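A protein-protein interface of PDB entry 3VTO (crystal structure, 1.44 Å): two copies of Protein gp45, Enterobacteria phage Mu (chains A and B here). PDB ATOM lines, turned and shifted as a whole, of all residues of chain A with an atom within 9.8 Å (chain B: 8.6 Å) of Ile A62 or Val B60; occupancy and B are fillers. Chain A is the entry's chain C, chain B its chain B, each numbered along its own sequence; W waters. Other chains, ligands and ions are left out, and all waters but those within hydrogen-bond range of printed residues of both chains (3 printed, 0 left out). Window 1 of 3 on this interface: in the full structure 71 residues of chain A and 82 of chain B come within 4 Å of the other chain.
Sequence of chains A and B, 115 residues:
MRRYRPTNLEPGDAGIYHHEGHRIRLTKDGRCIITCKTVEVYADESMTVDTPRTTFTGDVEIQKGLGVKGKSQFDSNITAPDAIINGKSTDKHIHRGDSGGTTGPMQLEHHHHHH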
ATOM      1  N   MET A  47       7.363 -12.300  -4.889  1.00  0.00           N
ATOM      2  CA  MET A  47       8.772 -12.244  -5.195  1.00  0.00           C
ATOM      3  C   MET A  47       9.303 -10.921  -4.706  1.00  0.00           C
ATOM      4  O   MET A  47       8.702  -9.872  -4.939  1.00  0.00           O
ATOM      5  CB  MET A  47       9.007 -12.416  -6.709  1.00  0.00           C
ATOM      6  CG  MET A  47      10.434 -12.211  -7.132  1.00  0.00           C
ATOM      7  SD  MET A  47      10.721 -12.919  -8.767  1.00  0.00           S
ATOM      8  CE  MET A  47      12.476 -12.549  -8.965  1.00  0.00           C
ATOM      9  N   VAL A  49      12.915  -8.656  -4.835  1.00  0.00           N
ATOM     10  CA  VAL A  49      14.267  -8.493  -5.340  1.00  0.00           C
ATOM     11  C   VAL A  49      14.879  -7.354  -4.563  1.00  0.00           C
ATOM     12  O   VAL A  49      14.489  -6.197  -4.721  1.00  0.00           O
ATOM     13  CB  VAL A  49      14.271  -8.154  -6.863  1.00  0.00           C
ATOM     14  CG1 VAL A  49      15.677  -7.837  -7.352  1.00  0.00           C
ATOM     15  CG2 VAL A  49      13.624  -9.277  -7.654  1.00  0.00           C
ATOM     16  N   THR A  54      18.262  -3.006 -10.268  1.00  0.00           N
ATOM     17  CA  THR A  54      17.872  -4.096 -11.142  1.00  0.00           C
ATOM     18  C   THR A  54      17.698  -3.538 -12.553  1.00  0.00           C
ATOM     19  O   THR A  54      16.968  -2.542 -12.726  1.00  0.00           O
ATOM     20  CB  THR A  54      16.554  -4.711 -10.692  1.00  0.00           C
ATOM     21  OG1 THR A  54      16.659  -5.177  -9.343  1.00  0.00           O
ATOM     22  CG2 THR A  54      16.155  -5.889 -11.579  1.00  0.00           C
ATOM     23  N   PHE A  56      16.632  -4.425 -16.603  1.00  0.00           N
ATOM     24  CA  PHE A  56      16.057  -5.313 -17.594  1.00  0.00           C
ATOM     25  C   PHE A  56      16.519  -4.795 -18.936  1.00  0.00           C
ATOM     26  O   PHE A  56      16.284  -3.637 -19.234  1.00  0.00           O
ATOM     27  CB  PHE A  56      14.522  -5.272 -17.510  1.00  0.00           C
ATOM     28  CG  PHE A  56      13.992  -5.795 -16.223  1.00  0.00           C
ATOM     29  CD1 PHE A  56      13.686  -7.154 -16.070  1.00  0.00           C
ATOM     30  CD2 PHE A  56      13.777  -4.945 -15.146  1.00  0.00           C
ATOM     31  CE1 PHE A  56      13.258  -7.650 -14.843  1.00  0.00           C
ATOM     32  CE2 PHE A  56      13.331  -5.433 -13.928  1.00  0.00           C
ATOM     33  CZ  PHE A  56      13.067  -6.791 -13.770  1.00  0.00           C
ATOM     34  N   ASP A  59      12.082  -5.449 -23.080  1.00  0.00           N
ATOM     35  CA  ASP A  59      10.786  -4.896 -22.706  1.00  0.00           C
ATOM     36  C   ASP A  59      10.322  -5.483 -21.383  1.00  0.00           C
ATOM     37  O   ASP A  59      10.714  -6.605 -21.036  1.00  0.00           O
ATOM     38  CB  ASP A  59       9.724  -5.242 -23.777  1.00  0.00           C
ATOM     39  CG  ASP A  59       9.987  -4.526 -25.115  1.00  0.00           C
ATOM     40  OD1 ASP A  59      10.276  -3.314 -25.122  1.00  0.00           O
ATOM     41  OD2 ASP A  59       9.933  -5.186 -26.179  1.00  0.00           O
ATOM     42  N   VAL A  60       9.464  -4.748 -20.676  1.00  0.00           N
ATOM     43  CA  VAL A  60       8.802  -5.239 -19.465  1.00  0.00           C
ATOM     44  C   VAL A  60       7.308  -5.023 -19.607  1.00  0.00           C
ATOM     45  O   VAL A  60       6.859  -3.965 -20.041  1.00  0.00           O
ATOM     46  CB  VAL A  60       9.363  -4.505 -18.213  1.00  0.00           C
ATOM     47  CG1 VAL A  60       8.581  -4.833 -16.944  1.00  0.00           C
ATOM     48  CG2 VAL A  60      10.855  -4.846 -17.997  1.00  0.00           C
ATOM     49  N   GLU A  61       6.573  -6.054 -19.270  1.00  0.00           N
ATOM     50  CA  GLU A  61       5.118  -6.006 -19.251  1.00  0.00           C
ATOM     51  C   GLU A  61       4.647  -6.305 -17.845  1.00  0.00           C
ATOM     52  O   GLU A  61       5.024  -7.334 -17.289  1.00  0.00           O
ATOM     53  CB  GLU A  61       4.526  -7.028 -20.226  1.00  0.00           C
ATOM     54  CG  GLU A  61       2.959  -7.133 -20.235  1.00  0.00           C
ATOM     55  CD  GLU A  61       2.391  -8.088 -21.286  1.00  0.00           C
ATOM     56  OE1 GLU A  61       2.924  -8.150 -22.426  1.00  0.00           O
ATOM     57  OE2 GLU A  61       1.369  -8.762 -20.997  1.00  0.00           O
ATOM     58  N   ILE A  62       3.810  -5.431 -17.278  1.00  0.00           N
ATOM     59  CA  ILE A  62       3.199  -5.641 -15.966  1.00  0.00           C
ATOM     60  C   ILE A  62       1.684  -5.781 -16.203  1.00  0.00           C
ATOM     61  O   ILE A  62       1.045  -4.866 -16.745  1.00  0.00           O
ATOM     62  CB  ILE A  62       3.531  -4.441 -15.029  1.00  0.00           C
ATOM     63  CG1 ILE A  62       5.074  -4.328 -14.847  1.00  0.00           C
ATOM     64  CG2 ILE A  62       2.815  -4.549 -13.700  1.00  0.00           C
ATOM     65  CD1 ILE A  62       5.537  -3.075 -14.142  1.00  0.00           C
ATOM     66  N   GLN A  63       1.129  -6.894 -15.751  1.00  0.00           N
ATOM     67  CA  GLN A  63      -0.258  -7.232 -16.123  1.00  0.00           C
ATOM     68  C   GLN A  63      -1.281  -6.709 -15.102  1.00  0.00           C
ATOM     69  O   GLN A  63      -2.466  -6.664 -15.412  1.00  0.00           O
ATOM     70  CB  GLN A  63      -0.370  -8.718 -16.366  1.00  0.00           C
ATOM     71  CG  GLN A  63       0.496  -9.162 -17.538  1.00  0.00           C
ATOM     72  CD  GLN A  63       0.280 -10.591 -17.940  1.00  0.00           C
ATOM     73  OE1 GLN A  63      -0.016 -11.444 -17.120  1.00  0.00           O
ATOM     74  NE2 GLN A  63       0.438 -10.863 -19.218  1.00  0.00           N
ATOM     75  N   LYS A  64      -0.830  -6.307 -13.927  1.00  0.00           N
ATOM     76  CA  LYS A  64      -1.679  -5.580 -12.978  1.00  0.00           C
ATOM     77  C   LYS A  64      -1.088  -4.198 -12.773  1.00  0.00           C
ATOM     78  O   LYS A  64      -0.798  -3.536 -13.765  1.00  0.00           O
ATOM     79  CB  LYS A  64      -1.963  -6.386 -11.701  1.00  0.00           C
ATOM     80  CG  LYS A  64      -2.642  -7.728 -12.042  1.00  0.00           C
ATOM     81  CD  LYS A  64      -3.237  -8.406 -10.843  1.00  0.00           C
ATOM     82  CE  LYS A  64      -4.126  -9.556 -11.324  1.00  0.00           C
ATOM     83  NZ  LYS A  64      -4.731 -10.332 -10.233  1.00  0.00           N
ATOM     84  N   GLY A  65      -1.003  -3.739 -11.537  1.00  0.00           N
ATOM     85  CA  GLY A  65      -0.578  -2.342 -11.293  1.00  0.00           C
ATOM     86  C   GLY A  65       0.892  -2.122 -11.012  1.00  0.00           C
ATOM     87  O   GLY A  65       1.602  -3.070 -10.700  1.00  0.00           O
ATOM     88  N   LEU A  66       1.289  -0.861 -11.047  1.00  0.00           N
ATOM     89  CA  LEU A  66       2.657  -0.448 -10.768  1.00  0.00           C
ATOM     90  C   LEU A  66       2.630   0.615  -9.699  1.00  0.00           C
ATOM     91  O   LEU A  66       1.847   1.563  -9.771  1.00  0.00           O
ATOM     92  CB  LEU A  66       3.306   0.129 -12.041  1.00  0.00           C
ATOM     93  CG  LEU A  66       4.673   0.780 -11.876  1.00  0.00           C
ATOM     94  CD1 LEU A  66       5.743  -0.232 -11.421  1.00  0.00           C
ATOM     95  CD2 LEU A  66       5.081   1.428 -13.174  1.00  0.00           C
ATOM     96  N   GLY A  67       3.557   0.521  -8.746  1.00  0.00           N
ATOM     97  CA  GLY A  67       3.739   1.567  -7.786  1.00  0.00           C
ATOM     98  C   GLY A  67       5.217   1.880  -7.740  1.00  0.00           C
ATOM     99  O   GLY A  67       6.024   0.938  -7.738  1.00  0.00           O
ATOM    100  N   VAL A  68       5.566   3.166  -7.747  1.00  0.00           N
ATOM    101  CA  VAL A  68       6.974   3.588  -7.658  1.00  0.00           C
ATOM    102  C   VAL A  68       7.093   4.638  -6.553  1.00  0.00           C
ATOM    103  O   VAL A  68       6.419   5.681  -6.604  1.00  0.00           O
ATOM    104  CB  VAL A  68       7.485   4.191  -9.009  1.00  0.00           C
ATOM    105  CG1 VAL A  68       8.939   4.601  -8.865  1.00  0.00           C
ATOM    106  CG2 VAL A  68       7.291   3.184 -10.156  1.00  0.00           C
ATOM    107  N   LYS A  69       7.973   4.401  -5.579  1.00  0.00           N
ATOM    108  CA  LYS A  69       8.149   5.361  -4.465  1.00  0.00           C
ATOM    109  C   LYS A  69       9.046   6.529  -4.808  1.00  0.00           C
ATOM    110  O   LYS A  69       8.737   7.659  -4.452  1.00  0.00           O
ATOM    111  CB  LYS A  69       8.671   4.651  -3.207  1.00  0.00           C
ATOM    112  CG  LYS A  69       7.636   3.682  -2.686  1.00  0.00           C
ATOM    113  CD  LYS A  69       8.075   3.137  -1.328  1.00  0.00           C
ATOM    114  CE  LYS A  69       6.914   2.553  -0.539  1.00  0.00           C
ATOM    115  NZ  LYS A  69       5.955   1.769  -1.376  1.00  0.00           N
ATOM    116  N   PHE A  74      11.535   8.890 -17.715  1.00  0.00           N
ATOM    117  CA  PHE A  74      11.183   8.229 -18.960  1.00  0.00           C
ATOM    118  C   PHE A  74      11.907   8.940 -20.100  1.00  0.00           C
ATOM    119  O   PHE A  74      11.730  10.141 -20.279  1.00  0.00           O
ATOM    120  CB  PHE A  74       9.664   8.290 -19.188  1.00  0.00           C
ATOM    121  CG  PHE A  74       8.866   7.608 -18.100  1.00  0.00           C
ATOM    122  CD1 PHE A  74       8.673   6.227 -18.130  1.00  0.00           C
ATOM    123  CD2 PHE A  74       8.314   8.335 -17.035  1.00  0.00           C
ATOM    124  CE1 PHE A  74       7.963   5.594 -17.128  1.00  0.00           C
ATOM    125  CE2 PHE A  74       7.555   7.693 -16.033  1.00  0.00           C
ATOM    126  CZ  PHE A  74       7.393   6.322 -16.084  1.00  0.00           C
ATOM    127  N   ARG B  53      12.036  -9.998 -23.317  1.00  0.00           N
ATOM    128  CA  ARG B  53      10.775  -9.606 -22.681  1.00  0.00           C
ATOM    129  C   ARG B  53      10.630 -10.253 -21.338  1.00  0.00           C
ATOM    130  O   ARG B  53      10.834 -11.465 -21.206  1.00  0.00           O
ATOM    131  CB  ARG B  53       9.567 -10.039 -23.526  1.00  0.00           C
ATOM    132  CG  ARG B  53       8.310  -9.339 -23.024  1.00  0.00           C
ATOM    133  CD  ARG B  53       7.058  -9.878 -23.717  1.00  0.00           C
ATOM    134  NE  ARG B  53       7.106  -9.719 -25.168  1.00  0.00           N
ATOM    135  CZ  ARG B  53       6.202 -10.248 -25.999  1.00  0.00           C
ATOM    136  NH1 ARG B  53       5.192 -10.968 -25.519  1.00  0.00           N
ATOM    137  NH2 ARG B  53       6.311 -10.064 -27.306  1.00  0.00           N
ATOM    138  N   THR B  54      10.300  -9.435 -20.343  1.00  0.00           N
ATOM    139  CA  THR B  54      10.037  -9.905 -18.980  1.00  0.00           C
ATOM    140  C   THR B  54       8.577  -9.564 -18.676  1.00  0.00           C
ATOM    141  O   THR B  54       8.170  -8.409 -18.885  1.00  0.00           O
ATOM    142  CB  THR B  54      10.965  -9.231 -17.948  1.00  0.00           C
ATOM    143  OG1 THR B  54      12.326  -9.499 -18.284  1.00  0.00           O
ATOM    144  CG2 THR B  54      10.688  -9.739 -16.572  1.00  0.00           C
ATOM    145  N   THR B  55       7.787 -10.551 -18.253  1.00  0.00           N
ATOM    146  CA  THR B  55       6.411 -10.322 -17.915  1.00  0.00           C
ATOM    147  C   THR B  55       6.156 -10.596 -16.456  1.00  0.00           C
ATOM    148  O   THR B  55       6.571 -11.614 -15.968  1.00  0.00           O
ATOM    149  CB  THR B  55       5.494 -11.200 -18.802  1.00  0.00           C
ATOM    150  OG1 THR B  55       5.743 -10.890 -20.177  1.00  0.00           O
ATOM    151  CG2 THR B  55       3.988 -10.933 -18.526  1.00  0.00           C
ATOM    152  N   PHE B  56       5.467  -9.681 -15.780  1.00  0.00           N
ATOM    153  CA  PHE B  56       4.984  -9.886 -14.403  1.00  0.00           C
ATOM    154  C   PHE B  56       3.463 -10.013 -14.466  1.00  0.00           C
ATOM    155  O   PHE B  56       2.775  -9.102 -14.984  1.00  0.00           O
ATOM    156  CB  PHE B  56       5.357  -8.692 -13.516  1.00  0.00           C
ATOM    157  CG  PHE B  56       6.823  -8.500 -13.407  1.00  0.00           C
ATOM    158  CD1 PHE B  56       7.528  -9.219 -12.455  1.00  0.00           C
ATOM    159  CD2 PHE B  56       7.508  -7.700 -14.319  1.00  0.00           C
ATOM    160  CE1 PHE B  56       8.933  -9.083 -12.348  1.00  0.00           C
ATOM    161  CE2 PHE B  56       8.887  -7.569 -14.238  1.00  0.00           C
ATOM    162  CZ  PHE B  56       9.609  -8.278 -13.274  1.00  0.00           C
ATOM    163  N   THR B  57       2.933 -11.107 -13.933  1.00  0.00           N
ATOM    164  CA  THR B  57       1.489 -11.336 -14.029  1.00  0.00           C
ATOM    165  C   THR B  57       0.683 -10.549 -12.971  1.00  0.00           C
ATOM    166  O   THR B  57      -0.553 -10.434 -13.057  1.00  0.00           O
ATOM    167  CB  THR B  57       1.128 -12.822 -13.850  1.00  0.00           C
ATOM    168  OG1 THR B  57       1.419 -13.219 -12.508  1.00  0.00           O
ATOM    169  CG2 THR B  57       1.834 -13.704 -14.885  1.00  0.00           C
ATOM    170  N   GLY B  58       1.367 -10.060 -11.951  1.00  0.00           N
ATOM    171  CA  GLY B  58       0.704  -9.391 -10.852  1.00  0.00           C
ATOM    172  C   GLY B  58       1.101  -7.927 -10.755  1.00  0.00           C
ATOM    173  O   GLY B  58       1.350  -7.278 -11.780  1.00  0.00           O
ATOM    174  N   ASP B  59       1.048  -7.392  -9.533  1.00  0.00           N
ATOM    175  CA  ASP B  59       1.484  -6.003  -9.248  1.00  0.00           C
ATOM    176  C   ASP B  59       2.988  -5.967  -9.100  1.00  0.00           C
ATOM    177  O   ASP B  59       3.603  -6.966  -8.751  1.00  0.00           O
ATOM    178  CB  ASP B  59       0.846  -5.493  -7.949  1.00  0.00           C
ATOM    179  CG  ASP B  59      -0.690  -5.364  -8.019  1.00  0.00           C
ATOM    180  OD1 ASP B  59      -1.201  -4.684  -8.935  1.00  0.00           O
ATOM    181  OD2 ASP B  59      -1.412  -5.894  -7.123  1.00  0.00           O
ATOM    182  N   VAL B  60       3.546  -4.808  -9.389  1.00  0.00           N
ATOM    183  CA  VAL B  60       4.953  -4.516  -9.162  1.00  0.00           C
ATOM    184  C   VAL B  60       5.046  -3.271  -8.298  1.00  0.00           C
ATOM    185  O   VAL B  60       4.372  -2.275  -8.558  1.00  0.00           O
ATOM    186  CB  VAL B  60       5.714  -4.315 -10.526  1.00  0.00           C
ATOM    187  CG1 VAL B  60       7.114  -3.794 -10.283  1.00  0.00           C
ATOM    188  CG2 VAL B  60       5.759  -5.606 -11.299  1.00  0.00           C
ATOM    189  N   GLU B  61       5.956  -3.305  -7.321  1.00  0.00           N
ATOM    190  CA  GLU B  61       6.252  -2.171  -6.460  1.00  0.00           C
ATOM    191  C   GLU B  61       7.742  -1.925  -6.549  1.00  0.00           C
ATOM    192  O   GLU B  61       8.530  -2.870  -6.370  1.00  0.00           O
ATOM    193  CB  GLU B  61       5.894  -2.444  -5.002  1.00  0.00           C
ATOM    194  CG  GLU B  61       6.335  -1.318  -4.039  1.00  0.00           C
ATOM    195  CD  GLU B  61       5.754  -1.455  -2.621  1.00  0.00           C
ATOM    196  OE1 GLU B  61       4.516  -1.649  -2.472  1.00  0.00           O
ATOM    197  OE2 GLU B  61       6.533  -1.351  -1.642  1.00  0.00           O
ATOM    198  N   ILE B  62       8.109  -0.688  -6.854  1.00  0.00           N
ATOM    199  CA  ILE B  62       9.514  -0.295  -6.890  1.00  0.00           C
ATOM    200  C   ILE B  62       9.740   0.711  -5.774  1.00  0.00           C
ATOM    201  O   ILE B  62       9.086   1.754  -5.737  1.00  0.00           O
ATOM    202  CB  ILE B  62       9.888   0.321  -8.300  1.00  0.00           C
ATOM    203  CG1 ILE B  62       9.736  -0.733  -9.395  1.00  0.00           C
ATOM    204  CG2 ILE B  62      11.278   0.881  -8.263  1.00  0.00           C
ATOM    205  CD1 ILE B  62       9.768  -0.195 -10.818  1.00  0.00           C
ATOM    206  N   GLN B  63      10.663   0.401  -4.856  1.00  0.00           N
ATOM    207  CA  GLN B  63      10.821   1.192  -3.632  1.00  0.00           C
ATOM    208  C   GLN B  63      11.751   2.387  -3.772  1.00  0.00           C
ATOM    209  O   GLN B  63      11.726   3.279  -2.920  1.00  0.00           O
ATOM    210  CB  GLN B  63      11.183   0.285  -2.428  1.00  0.00           C
ATOM    211  CG  GLN B  63      10.025  -0.719  -2.213  1.00  0.00           C
ATOM    212  CD  GLN B  63      10.197  -1.631  -0.980  1.00  0.00           C
ATOM    213  OE1 GLN B  63       9.207  -2.179  -0.454  1.00  0.00           O
ATOM    214  NE2 GLN B  63      11.416  -1.782  -0.522  1.00  0.00           N
ATOM    215  N   LEU B  66      12.699   4.635 -10.863  1.00  0.00           N
ATOM    216  CA  LEU B  66      12.471   3.888 -12.102  1.00  0.00           C
ATOM    217  C   LEU B  66      13.062   4.705 -13.248  1.00  0.00           C
ATOM    218  O   LEU B  66      12.812   5.913 -13.325  1.00  0.00           O
ATOM    219  CB  LEU B  66      10.966   3.698 -12.337  1.00  0.00           C
ATOM    220  CG  LEU B  66      10.546   3.153 -13.701  1.00  0.00           C
ATOM    221  CD1 LEU B  66      11.136   1.761 -13.979  1.00  0.00           C
ATOM    222  CD2 LEU B  66       9.031   3.138 -13.866  1.00  0.00           C
ATOM    223  N   GLN B  73       3.691   2.504 -22.275  1.00  0.00           N
ATOM    224  CA  GLN B  73       2.264   2.513 -22.515  1.00  0.00           C
ATOM    225  C   GLN B  73       1.551   2.108 -21.233  1.00  0.00           C
ATOM    226  O   GLN B  73       1.721   0.960 -20.765  1.00  0.00           O
ATOM    227  CB  GLN B  73       1.942   1.564 -23.648  1.00  0.00           C
ATOM    228  CG  GLN B  73       0.436   1.428 -23.862  1.00  0.00           C
ATOM    229  CD  GLN B  73       0.114   0.725 -25.150  1.00  0.00           C
ATOM    230  OE1 GLN B  73       0.785   0.943 -26.163  1.00  0.00           O
ATOM    231  NE2 GLN B  73      -0.930  -0.118 -25.138  1.00  0.00           N
ATOM    232  N   PHE B  74       0.747   3.025 -20.681  1.00  0.00           N
ATOM    233  CA  PHE B  74      -0.038   2.769 -19.491  1.00  0.00           C
ATOM    234  C   PHE B  74      -1.494   2.647 -19.914  1.00  0.00           C
ATOM    235  O   PHE B  74      -2.037   3.608 -20.477  1.00  0.00           O
ATOM    236  CB  PHE B  74       0.117   3.926 -18.512  1.00  0.00           C
ATOM    237  CG  PHE B  74       1.546   4.132 -18.043  1.00  0.00           C
ATOM    238  CD1 PHE B  74       2.085   3.349 -17.026  1.00  0.00           C
ATOM    239  CD2 PHE B  74       2.356   5.083 -18.648  1.00  0.00           C
ATOM    240  CE1 PHE B  74       3.408   3.570 -16.596  1.00  0.00           C
ATOM    241  CE2 PHE B  74       3.652   5.305 -18.207  1.00  0.00           C
ATOM    242  CZ  PHE B  74       4.185   4.512 -17.221  1.00  0.00           C
ATOM    243  N   ASP B  75      -2.094   1.479 -19.697  1.00  0.00           N
ATOM    244  CA  ASP B  75      -3.485   1.234 -20.175  1.00  0.00           C
ATOM    245  C   ASP B  75      -4.543   1.784 -19.255  1.00  0.00           C
ATOM    246  O   ASP B  75      -5.683   1.915 -19.667  1.00  0.00           O
ATOM    247  CB  ASP B  75      -3.746  -0.251 -20.387  1.00  0.00           C
ATOM    248  CG  ASP B  75      -2.843  -0.884 -21.449  1.00  0.00           C
ATOM    249  OD1 ASP B  75      -2.206  -0.183 -22.268  1.00  0.00           O
ATOM    250  OD2 ASP B  75      -2.759  -2.130 -21.441  1.00  0.00           O
HETATM  251  O   HOH W   1       8.531  -7.371 -26.269  1.00  0.00           O
HETATM  252  O   HOH W   2      13.315  -7.698 -20.451  1.00  0.00           O
HETATM  253  O   HOH W   3       3.965 -10.634 -22.271  1.00  0.00           O
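The side-chain carboxylate (OE2) of Glu A61 sits at hydrogen-bond distance from the side-chain amide nitrogen (NE2) of Gln A63 (2.9 Å). OE2 of Glu B61 sits close to OE1 of Gln B63, 3.0 Å away.
Of the 16 printed residues of chain A, 13 touch a printed residue of chain B. Hydrophobic or aromatic side chains of chain A that line the printed part of chain B: Phe A56, Val A60, Ile A62, Leu A66 and Phe A74. Hydrophobic or aromatic side chains of chain B within 4 Å of the printed part of chain A: Phe B56, Val B60, Ile B62 and Phe B74.
Asp A59 touches Thr B54, but with the chains exchanged Thr A54 does not touch Asp B59 (12.9 Å). Val A60 touches Thr B54, but with the chains exchanged Thr A54 does not touch Val B60 (9.4 Å). Glu A61 touches Phe B56, but with the chains exchanged Phe A56 does not touch Glu B61 (9.3 Å). Gln A63 touches Phe B56, but with the chains exchanged Phe A56 does not touch Gln B63 (11.1 Å). Of the 30 pairs that touch across the chains among the printed residues, 2 have their exchanged pair printed and touching as well.
Printed residues of chain B within 4 Å of Phe A56: Thr B54 and Phe B56. Of the printed residues of chain B, Val A60 touches Thr B54 and Phe B56. Of chain B, only Phe B56, Gly B58 and Val B60 come within 4 Å of Ile A62. Of the printed residues of chain B, Gln A63 touches Thr B55, Phe B56, Thr B57 and Gly B58. Of the printed residues of chain B, Gly A67 touches Val B60 (2.9 Å), Glu B61 (3.4 Å) and Ile B62 (2.8 Å). Asp B59 touches just these residues of chain A: Lys A64 (3.3 Å) and Gly A65 (2.8 Å). Val B60 touches just these residues of chain A: Ile A62 (3.8 Å), Gly A65 (2.9 Å), Leu A66 (3.3 Å) and Gly A67 (2.9 Å). The nearest residue of chain B that does not touch Ile A62 is Asp B59 (4.8 Å). The nearest printed residue of chain A that does not touch Thr B57 is Glu A61 (5.5 Å).
Among the printed residues, pairs that only touch across the chains: Phe A56 with Thr B54 (3.5 Å), Phe A56 with Phe B56 (3.8 Å), Asp A59 with Arg B53 (3.4 Å), Val A60 with Thr B54 (3.3 Å), Val A60 with Phe B56 (3.9 Å), Glu A61 with Thr B55 (3.4 Å), Ile A62 with Phe B56 (3.6 Å), Ile A62 with Gly B58 (3.6 Å), Ile A62 with Val B60 (3.8 Å), Gln A63 with Thr B55 (3.6 Å), Gln A63 with Thr B57 (3.4 Å), Gln A63 with Gly B58 (3.996 Å), Lys A64 with Thr B57 (3.6 Å), Lys A64 with Asp B59 (3.3 Å), Leu A66 with Val B60 (3.3 Å), Gly A67 with Glu B61 (3.4 Å), Val A68 with Ile B62 (3.4 Å), Lys A69 with Gln B63 (3.4 Å) and Phe A74 with Phe B74 (3.9 Å).
Water W1 lies within hydrogen-bond range of OD2 of Asp A59 (2.6 Å) and NE of Arg B53 (3.0 Å). Water W3 lies within hydrogen-bond range of OE1 of Glu A61 (2.7 Å), OG1 of Thr B55 (2.8 Å) and NH1 of Arg B53 (3.5 Å). Water W2 bridges O of Asp A59 (2.9 Å) and OG1 of Thr B54 (3.0 Å).
O of Glu A61 is in hydrogen-bond range of N of Phe B56 (2.8 Å). The backbone NH (N) of Thr B54 is in hydrogen-bond range of the backbone carbonyl oxygen (O) of Asp A59. The backbone NH (N) of Val B60 sits at hydrogen-bond distance from the backbone carbonyl oxygen (O) of Gly A65 (2.9 Å). N of Gln A63 sits at hydrogen-bond distance from O of Phe B56 (2.9 Å). O of Gly B58 lies within hydrogen-bond range of N of Lys A64 (3.2 Å). The backbone carbonyl oxygen (O) of Ile B62 lies within hydrogen-bond range of the backbone NH (N) of Lys A69 (2.9 Å). The side-chain amino group (NZ) of Lys A69 is in salt-bridge range of the side-chain carboxylate (OE2) of Glu B61, at 3.2 Å. The backbone NH (N) of Glu A61 lies within hydrogen-bond range of the backbone carbonyl oxygen (O) of Thr B54, at 2.9 Å. OD1 of Asp B59 lies within hydrogen-bond range of N of Gly A65 (2.8 Å). O of Gly A67 lies within hydrogen-bond range of N of Ile B62 (2.8 Å). The backbone carbonyl oxygen (O) of Val B60 is in hydrogen-bond range of the backbone NH (N) of Gly A67.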
